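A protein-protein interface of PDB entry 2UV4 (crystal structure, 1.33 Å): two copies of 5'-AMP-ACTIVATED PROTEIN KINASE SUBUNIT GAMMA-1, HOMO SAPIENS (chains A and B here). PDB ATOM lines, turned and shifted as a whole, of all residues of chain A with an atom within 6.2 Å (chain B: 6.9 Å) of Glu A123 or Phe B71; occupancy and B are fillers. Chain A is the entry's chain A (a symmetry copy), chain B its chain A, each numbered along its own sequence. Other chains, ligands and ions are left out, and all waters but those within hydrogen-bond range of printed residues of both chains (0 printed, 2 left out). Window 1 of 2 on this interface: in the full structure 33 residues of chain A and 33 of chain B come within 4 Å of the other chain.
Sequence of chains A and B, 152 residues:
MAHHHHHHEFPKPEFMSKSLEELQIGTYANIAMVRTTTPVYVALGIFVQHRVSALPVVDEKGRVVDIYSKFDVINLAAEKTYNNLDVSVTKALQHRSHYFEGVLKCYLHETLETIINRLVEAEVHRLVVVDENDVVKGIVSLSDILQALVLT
The side-chain hydroxyl (OG) of Ser B69 sits close to the backbone NH (N) of Phe B71, at 3.3 Å. The backbone carbonyl oxygen of Leu A119 is in hydrogen-bond range of the backbone NH of Val A124, 3.0 Å away. O of His A125 sits at hydrogen-bond distance from N of Leu A142, 3.1 Å away.
O of Leu A119 touches CE1 of Phe B71 (3.9 Å). CG2 of Ile B74 touches CG2 of Val A120, 3.7 Å away. CG1 of Val A120 touches OD1 of Asn B75, at 3.2 Å. Glu A123 touches Phe B71. NE2 of His A125 touches CB of Phe B71, 3.9 Å away. CE1 of His A125 touches CE1 of His B125, 3.3 Å away. N of Phe B71 touches CD1 of Leu A142, at 3.6 Å. CG1 of Ile B74 touches CD2 of Leu A142, at 3.9 Å.
Of chain B, only Phe B71 (3.8 Å) comes within 4 Å of Glu A123. Of chain A, only Leu A119, Glu A123, His A125 and Leu A142 come within 4 Å of Phe B71. Of the printed residues of chain A, Asn B75 touches Val A120 (3.2 Å). Of the printed residues of chain A, His B125 touches His A125 (3.3 Å). The nearest printed residue of chain B that does not touch Val A120 is Phe B71 (4.1 Å).
His A125 touches its own counterpart, His B125. 3 positions are printed for both chains. Of the 8 pairs that touch across the chains among the printed residues, 1 has its exchanged pair printed and touching as well.
Of the 9 printed residues of chain A, 5 touch a printed residue of chain B. Printed residues of chain A that touch a printed residue of chain B: Leu A119, Val A120, Glu A123, His A125 and Leu A142. Hydrophobic or aromatic side chains of chain A that line the printed part of chain B: Val A120, His A125 and Leu A142. Printed residues of chain B that touch a printed residue of chain A: Phe B71, Ile B74, Asn B75 and His B125. Hydrophobic or aromatic side chains of chain B within 4 Å of the printed part of chain A: Phe B71, Ile B74 and His B125.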
ATOM      1  N   ARG A 118      -7.331 -15.140  23.184  1.00  0.00           N
ATOM      2  CA  ARG A 118      -7.380 -15.003  21.730  1.00  0.00           C
ATOM      3  C   ARG A 118      -7.179 -13.553  21.328  1.00  0.00           C
ATOM      4  O   ARG A 118      -6.447 -13.257  20.388  1.00  0.00           O
ATOM      5  CB  ARG A 118      -8.708 -15.525  21.218  1.00  0.00           C
ATOM      6  CG  ARG A 118      -8.888 -15.511  19.689  1.00  0.00           C
ATOM      7  CD  ARG A 118     -10.197 -16.173  19.250  1.00  0.00           C
ATOM      8  NE  ARG A 118     -10.238 -17.547  19.677  1.00  0.00           N
ATOM      9  CZ  ARG A 118     -11.310 -18.217  20.035  1.00  0.00           C
ATOM     10  NH1 ARG A 118     -12.511 -17.685  19.920  1.00  0.00           N
ATOM     11  NH2 ARG A 118     -11.191 -19.456  20.521  1.00  0.00           N
ATOM     12  N   LEU A 119      -7.799 -12.612  22.048  1.00  0.00           N
ATOM     13  CA  LEU A 119      -7.565 -11.188  21.806  1.00  0.00           C
ATOM     14  C   LEU A 119      -6.096 -10.837  21.962  1.00  0.00           C
ATOM     15  O   LEU A 119      -5.520 -10.088  21.151  1.00  0.00           O
ATOM     16  CB  LEU A 119      -8.376 -10.343  22.796  1.00  0.00           C
ATOM     17  CG  LEU A 119      -9.894 -10.378  22.612  1.00  0.00           C
ATOM     18  CD1 LEU A 119     -10.589  -9.802  23.858  1.00  0.00           C
ATOM     19  CD2 LEU A 119     -10.316  -9.623  21.374  1.00  0.00           C
ATOM     20  N   VAL A 120      -5.475 -11.378  22.997  1.00  0.00           N
ATOM     21  CA  VAL A 120      -4.093 -10.992  23.278  1.00  0.00           C
ATOM     22  C   VAL A 120      -3.114 -11.651  22.313  1.00  0.00           C
ATOM     23  O   VAL A 120      -2.118 -11.026  21.955  1.00  0.00           O
ATOM     24  CB  VAL A 120      -3.773 -11.288  24.756  1.00  0.00           C
ATOM     25  CG1 VAL A 120      -2.288 -11.195  25.055  1.00  0.00           C
ATOM     26  CG2 VAL A 120      -4.578 -10.339  25.643  1.00  0.00           C
ATOM     27  N   GLU A 121      -3.407 -12.869  21.852  1.00  0.00           N
ATOM     28  CA  GLU A 121      -2.536 -13.575  20.901  1.00  0.00           C
ATOM     29  C   GLU A 121      -2.150 -12.728  19.693  1.00  0.00           C
ATOM     30  O   GLU A 121      -1.001 -12.770  19.249  1.00  0.00           O
ATOM     31  CB  GLU A 121      -3.215 -14.849  20.419  1.00  0.00           C
ATOM     32  CG  GLU A 121      -2.365 -15.713  19.482  1.00  0.00           C
ATOM     33  CD  GLU A 121      -1.188 -16.371  20.179  1.00  0.00           C
ATOM     34  OE1 GLU A 121      -1.038 -16.202  21.415  1.00  0.00           O
ATOM     35  OE2 GLU A 121      -0.406 -17.069  19.487  1.00  0.00           O
ATOM     36  N   ALA A 122      -3.104 -11.994  19.128  1.00  0.00           N
ATOM     37  CA  ALA A 122      -2.851 -11.202  17.922  1.00  0.00           C
ATOM     38  C   ALA A 122      -2.970  -9.717  18.164  1.00  0.00           C
ATOM     39  O   ALA A 122      -2.894  -8.930  17.235  1.00  0.00           O
ATOM     40  CB  ALA A 122      -3.807 -11.613  16.797  1.00  0.00           C
ATOM     41  N   GLU A 123      -3.127  -9.322  19.423  1.00  0.00           N
ATOM     42  CA  GLU A 123      -3.342  -7.947  19.766  1.00  0.00           C
ATOM     43  C   GLU A 123      -4.468  -7.378  18.946  1.00  0.00           C
ATOM     44  O   GLU A 123      -4.291  -6.393  18.211  1.00  0.00           O
ATOM     45  CB  GLU A 123      -2.077  -7.113  19.567  1.00  0.00           C
ATOM     46  CG  GLU A 123      -0.860  -7.601  20.310  1.00  0.00           C
ATOM     47  CD  GLU A 123       0.296  -6.651  20.079  1.00  0.00           C
ATOM     48  OE1 GLU A 123       0.203  -5.497  20.567  1.00  0.00           O
ATOM     49  OE2 GLU A 123       1.252  -7.047  19.378  1.00  0.00           O
ATOM     50  N   VAL A 124      -5.640  -7.980  19.083  1.00  0.00           N
ATOM     51  CA  VAL A 124      -6.830  -7.445  18.424  1.00  0.00           C
ATOM     52  C   VAL A 124      -7.799  -6.983  19.462  1.00  0.00           C
ATOM     53  O   VAL A 124      -7.687  -7.371  20.621  1.00  0.00           O
ATOM     54  CB  VAL A 124      -7.503  -8.454  17.460  1.00  0.00           C
ATOM     55  CG1 VAL A 124      -6.564  -8.731  16.274  1.00  0.00           C
ATOM     56  CG2 VAL A 124      -7.908  -9.750  18.166  1.00  0.00           C
ATOM     57  N   HIS A 125      -8.717  -6.100  19.082  1.00  0.00           N
ATOM     58  CA  HIS A 125      -9.551  -5.414  20.057  1.00  0.00           C
ATOM     59  C   HIS A 125     -11.009  -5.890  20.089  1.00  0.00           C
ATOM     60  O   HIS A 125     -11.787  -5.388  20.874  1.00  0.00           O
ATOM     61  CB  HIS A 125      -9.528  -3.907  19.816  1.00  0.00           C
ATOM     62  CG  HIS A 125      -8.189  -3.274  20.055  1.00  0.00           C
ATOM     63  ND1 HIS A 125      -8.018  -1.910  20.064  1.00  0.00           N
ATOM     64  CD2 HIS A 125      -6.978  -3.811  20.345  1.00  0.00           C
ATOM     65  CE1 HIS A 125      -6.747  -1.634  20.327  1.00  0.00           C
ATOM     66  NE2 HIS A 125      -6.092  -2.768  20.484  1.00  0.00           N
ATOM     67  N   LEU A 142     -13.106  -4.992  23.693  1.00  0.00           N
ATOM     68  CA  LEU A 142     -12.433  -4.837  24.986  1.00  0.00           C
ATOM     69  C   LEU A 142     -13.347  -4.089  25.947  1.00  0.00           C
ATOM     70  O   LEU A 142     -13.375  -4.421  27.117  1.00  0.00           O
ATOM     71  CB  LEU A 142     -11.113  -4.090  24.863  1.00  0.00           C
ATOM     72  CG  LEU A 142     -10.159  -4.535  23.774  1.00  0.00           C
ATOM     73  CD1 LEU A 142      -8.930  -3.614  23.753  1.00  0.00           C
ATOM     74  CD2 LEU A 142      -9.767  -5.983  23.979  1.00  0.00           C
ATOM     75  N   PHE B  47     -11.902   3.788  32.650  1.00  0.00           N
ATOM     76  CA  PHE B  47     -12.330   3.264  31.362  1.00  0.00           C
ATOM     77  C   PHE B  47     -13.808   2.913  31.366  1.00  0.00           C
ATOM     78  O   PHE B  47     -14.488   3.190  30.361  1.00  0.00           O
ATOM     79  CB  PHE B  47     -11.518   2.015  30.991  1.00  0.00           C
ATOM     80  CG  PHE B  47     -10.064   2.295  30.607  1.00  0.00           C
ATOM     81  CD1 PHE B  47      -9.730   3.351  29.804  1.00  0.00           C
ATOM     82  CD2 PHE B  47      -9.061   1.422  30.987  1.00  0.00           C
ATOM     83  CE1 PHE B  47      -8.449   3.574  29.439  1.00  0.00           C
ATOM     84  CE2 PHE B  47      -7.753   1.665  30.609  1.00  0.00           C
ATOM     85  CZ  PHE B  47      -7.449   2.732  29.848  1.00  0.00           C
ATOM     86  N   SER B  53     -10.756   5.953  25.791  1.00  0.00           N
ATOM     87  CA  SER B  53     -10.107   4.744  25.266  1.00  0.00           C
ATOM     88  C   SER B  53      -8.671   4.533  25.767  1.00  0.00           C
ATOM     89  O   SER B  53      -8.172   3.385  25.823  1.00  0.00           O
ATOM     90  CB  SER B  53     -10.145   4.762  23.741  1.00  0.00           C
ATOM     91  OG  SER B  53      -9.593   5.962  23.233  1.00  0.00           O
ATOM     92  N   TYR B  68      -1.745   4.438  28.516  1.00  0.00           N
ATOM     93  CA  TYR B  68      -2.306   3.196  29.040  1.00  0.00           C
ATOM     94  C   TYR B  68      -3.668   3.008  28.443  1.00  0.00           C
ATOM     95  O   TYR B  68      -4.502   3.888  28.549  1.00  0.00           O
ATOM     96  CB  TYR B  68      -2.381   3.285  30.569  1.00  0.00           C
ATOM     97  CG  TYR B  68      -2.665   1.970  31.225  1.00  0.00           C
ATOM     98  CD1 TYR B  68      -1.652   1.072  31.499  1.00  0.00           C
ATOM     99  CD2 TYR B  68      -3.926   1.653  31.641  1.00  0.00           C
ATOM    100  CE1 TYR B  68      -1.910  -0.110  32.103  1.00  0.00           C
ATOM    101  CE2 TYR B  68      -4.177   0.443  32.239  1.00  0.00           C
ATOM    102  CZ  TYR B  68      -3.161  -0.458  32.474  1.00  0.00           C
ATOM    103  OH  TYR B  68      -3.428  -1.674  33.066  1.00  0.00           O
ATOM    104  N   SER B  69      -3.909   1.865  27.807  1.00  0.00           N
ATOM    105  CA  SER B  69      -5.118   1.623  27.018  1.00  0.00           C
ATOM    106  C   SER B  69      -5.908   0.446  27.538  1.00  0.00           C
ATOM    107  O   SER B  69      -5.467  -0.293  28.419  1.00  0.00           O
ATOM    108  CB  SER B  69      -4.746   1.321  25.606  1.00  0.00           C
ATOM    109  OG  SER B  69      -4.184   0.015  25.541  1.00  0.00           O
ATOM    110  N   LYS B  70      -7.138   0.319  27.025  1.00  0.00           N
ATOM    111  CA  LYS B  70      -7.977  -0.813  27.402  1.00  0.00           C
ATOM    112  C   LYS B  70      -7.262  -2.120  27.106  1.00  0.00           C
ATOM    113  O   LYS B  70      -7.379  -3.109  27.852  1.00  0.00           O
ATOM    114  CB  LYS B  70      -9.330  -0.744  26.682  1.00  0.00           C
ATOM    115  CG  LYS B  70     -10.175   0.399  27.202  1.00  0.00           C
ATOM    116  CD  LYS B  70     -11.510   0.554  26.450  1.00  0.00           C
ATOM    117  CE  LYS B  70     -12.354   1.677  26.980  1.00  0.00           C
ATOM    118  NZ  LYS B  70     -13.603   1.879  26.113  1.00  0.00           N
ATOM    119  N   PHE B  71      -6.544  -2.178  25.989  1.00  0.00           N
ATOM    120  CA  PHE B  71      -5.833  -3.379  25.653  1.00  0.00           C
ATOM    121  C   PHE B  71      -4.789  -3.711  26.716  1.00  0.00           C
ATOM    122  O   PHE B  71      -4.576  -4.881  27.012  1.00  0.00           O
ATOM    123  CB  PHE B  71      -5.193  -3.318  24.262  1.00  0.00           C
ATOM    124  CG  PHE B  71      -4.481  -4.599  23.901  1.00  0.00           C
ATOM    125  CD1 PHE B  71      -5.201  -5.704  23.473  1.00  0.00           C
ATOM    126  CD2 PHE B  71      -3.128  -4.745  24.121  1.00  0.00           C
ATOM    127  CE1 PHE B  71      -4.573  -6.914  23.205  1.00  0.00           C
ATOM    128  CE2 PHE B  71      -2.496  -5.946  23.852  1.00  0.00           C
ATOM    129  CZ  PHE B  71      -3.216  -7.031  23.409  1.00  0.00           C
ATOM    130  N   ASP B  72      -4.169  -2.705  27.308  1.00  0.00           N
ATOM    131  CA  ASP B  72      -3.186  -2.991  28.354  1.00  0.00           C
ATOM    132  C   ASP B  72      -3.828  -3.685  29.514  1.00  0.00           C
ATOM    133  O   ASP B  72      -3.200  -4.532  30.163  1.00  0.00           O
ATOM    134  CB  ASP B  72      -2.512  -1.703  28.814  1.00  0.00           C
ATOM    135  CG  ASP B  72      -1.646  -1.091  27.741  1.00  0.00           C
ATOM    136  OD1 ASP B  72      -0.929  -1.833  27.027  1.00  0.00           O
ATOM    137  OD2 ASP B  72      -1.615   0.144  27.575  1.00  0.00           O
ATOM    138  N   VAL B  73      -5.073  -3.371  29.832  1.00  0.00           N
ATOM    139  CA  VAL B  73      -5.731  -4.041  30.922  1.00  0.00           C
ATOM    140  C   VAL B  73      -5.984  -5.484  30.567  1.00  0.00           C
ATOM    141  O   VAL B  73      -5.829  -6.376  31.402  1.00  0.00           O
ATOM    142  CB  VAL B  73      -7.093  -3.370  31.319  1.00  0.00           C
ATOM    143  CG1 VAL B  73      -7.812  -4.143  32.424  1.00  0.00           C
ATOM    144  CG2 VAL B  73      -6.831  -1.971  31.781  1.00  0.00           C
ATOM    145  N   ILE B  74      -6.404  -5.742  29.335  1.00  0.00           N
ATOM    146  CA  ILE B  74      -6.695  -7.087  28.889  1.00  0.00           C
ATOM    147  C   ILE B  74      -5.421  -7.910  28.828  1.00  0.00           C
ATOM    148  O   ILE B  74      -5.412  -9.085  29.177  1.00  0.00           O
ATOM    149  CB  ILE B  74      -7.411  -7.052  27.527  1.00  0.00           C
ATOM    150  CG1 ILE B  74      -8.768  -6.340  27.680  1.00  0.00           C
ATOM    151  CG2 ILE B  74      -7.546  -8.495  26.925  1.00  0.00           C
ATOM    152  CD1 ILE B  74      -9.696  -6.989  28.626  1.00  0.00           C
ATOM    153  N   ASN B  75      -4.326  -7.274  28.420  1.00  0.00           N
ATOM    154  CA  ASN B  75      -3.029  -7.929  28.422  1.00  0.00           C
ATOM    155  C   ASN B  75      -2.622  -8.314  29.847  1.00  0.00           C
ATOM    156  O   ASN B  75      -2.156  -9.424  30.047  1.00  0.00           O
ATOM    157  CB  ASN B  75      -1.994  -7.030  27.726  1.00  0.00           C
ATOM    158  CG  ASN B  75      -0.869  -7.792  27.058  1.00  0.00           C
ATOM    159  OD1 ASN B  75      -0.916  -9.011  26.904  1.00  0.00           O
ATOM    160  ND2 ASN B  75       0.143  -7.066  26.645  1.00  0.00           N
ATOM    161  N   LEU B  76      -2.800  -7.421  30.810  1.00  0.00           N
ATOM    162  CA  LEU B  76      -2.569  -7.766  32.189  1.00  0.00           C
ATOM    163  C   LEU B  76      -3.427  -8.968  32.585  1.00  0.00           C
ATOM    164  O   LEU B  76      -2.954  -9.908  33.268  1.00  0.00           O
ATOM    165  CB  LEU B  76      -2.888  -6.558  33.082  1.00  0.00           C
ATOM    166  CG  LEU B  76      -2.726  -6.769  34.585  1.00  0.00           C
ATOM    167  CD1 LEU B  76      -1.264  -6.965  35.002  1.00  0.00           C
ATOM    168  CD2 LEU B  76      -3.298  -5.546  35.322  1.00  0.00           C
ATOM    169  N   ALA B  77      -4.701  -8.960  32.222  1.00  0.00           N
ATOM    170  CA  ALA B  77      -5.592 -10.028  32.601  1.00  0.00           C
ATOM    171  C   ALA B  77      -5.134 -11.355  32.084  1.00  0.00           C
ATOM    172  O   ALA B  77      -5.395 -12.372  32.722  1.00  0.00           O
ATOM    173  CB  ALA B  77      -7.048  -9.714  32.119  1.00  0.00           C
ATOM    174  N   ARG B  96       5.823  -3.409  26.219  1.00  0.00           N
ATOM    175  CA  ARG B  96       6.016  -2.469  25.124  1.00  0.00           C
ATOM    176  C   ARG B  96       6.450  -1.137  25.682  1.00  0.00           C
ATOM    177  O   ARG B  96       6.037  -0.741  26.799  1.00  0.00           O
ATOM    178  CB  ARG B  96       4.736  -2.281  24.280  1.00  0.00           C
ATOM    179  CG  ARG B  96       3.623  -1.380  24.826  1.00  0.00           C
ATOM    180  CD  ARG B  96       2.959  -1.932  26.105  1.00  0.00           C
ATOM    181  NE  ARG B  96       1.921  -1.035  26.600  1.00  0.00           N
ATOM    182  CZ  ARG B  96       2.185   0.096  27.228  1.00  0.00           C
ATOM    183  NH1 ARG B  96       3.427   0.502  27.429  1.00  0.00           N
ATOM    184  NH2 ARG B  96       1.213   0.850  27.658  1.00  0.00           N
ATOM    185  N   ALA B 122       3.949   1.348  14.545  1.00  0.00           N
ATOM    186  CA  ALA B 122       3.831   0.472  15.713  1.00  0.00           C
ATOM    187  C   ALA B 122       2.432  -0.063  15.901  1.00  0.00           C
ATOM    188  O   ALA B 122       2.148  -0.720  16.889  1.00  0.00           O
ATOM    189  CB  ALA B 122       4.271   1.205  16.984  1.00  0.00           C
ATOM    190  N   GLU B 123       1.555   0.189  14.935  1.00  0.00           N
ATOM    191  CA  GLU B 123       0.176  -0.188  15.044  1.00  0.00           C
ATOM    192  C   GLU B 123      -0.395   0.305  16.346  1.00  0.00           C
ATOM    193  O   GLU B 123      -0.887  -0.483  17.171  1.00  0.00           O
ATOM    194  CB  GLU B 123      -0.004  -1.702  14.936  1.00  0.00           C
ATOM    195  CG  GLU B 123       0.562  -2.330  13.687  1.00  0.00           C
ATOM    196  CD  GLU B 123       0.257  -3.812  13.677  1.00  0.00           C
ATOM    197  OE1 GLU B 123      -0.946  -4.156  13.556  1.00  0.00           O
ATOM    198  OE2 GLU B 123       1.207  -4.609  13.838  1.00  0.00           O
ATOM    199  N   HIS B 125      -3.057   3.354  18.170  1.00  0.00           N
ATOM    200  CA  HIS B 125      -4.315   3.977  17.789  1.00  0.00           C
ATOM    201  C   HIS B 125      -4.445   5.448  18.207  1.00  0.00           C
ATOM    202  O   HIS B 125      -5.453   6.063  17.928  1.00  0.00           O
ATOM    203  CB  HIS B 125      -5.495   3.195  18.358  1.00  0.00           C
ATOM    204  CG  HIS B 125      -5.646   1.818  17.781  1.00  0.00           C
ATOM    205  ND1 HIS B 125      -6.748   1.037  18.036  1.00  0.00           N
ATOM    206  CD2 HIS B 125      -4.867   1.109  16.927  1.00  0.00           C
ATOM    207  CE1 HIS B 125      -6.629  -0.109  17.379  1.00  0.00           C
ATOM    208  NE2 HIS B 125      -5.490  -0.099  16.713  1.00  0.00           N
ATOM    209  N   ARG B 126      -3.469   5.949  18.955  1.00  0.00           N
ATOM    210  CA  ARG B 126      -3.469   7.353  19.308  1.00  0.00           C
ATOM    211  C   ARG B 126      -2.087   7.802  19.645  1.00  0.00           C
ATOM    212  O   ARG B 126      -1.215   6.986  19.931  1.00  0.00           O
ATOM    213  CB  ARG B 126      -4.413   7.639  20.462  1.00  0.00           C
ATOM    214  CG  ARG B 126      -3.986   7.209  21.809  1.00  0.00           C
ATOM    215  CD  ARG B 126      -4.002   5.737  22.027  1.00  0.00           C
ATOM    216  NE  ARG B 126      -5.320   5.168  21.876  1.00  0.00           N
ATOM    217  CZ  ARG B 126      -5.613   3.900  22.112  1.00  0.00           C
ATOM    218  NH1 ARG B 126      -4.649   3.074  22.472  1.00  0.00           N
ATOM    219  NH2 ARG B 126      -6.864   3.462  21.979  1.00  0.00           N
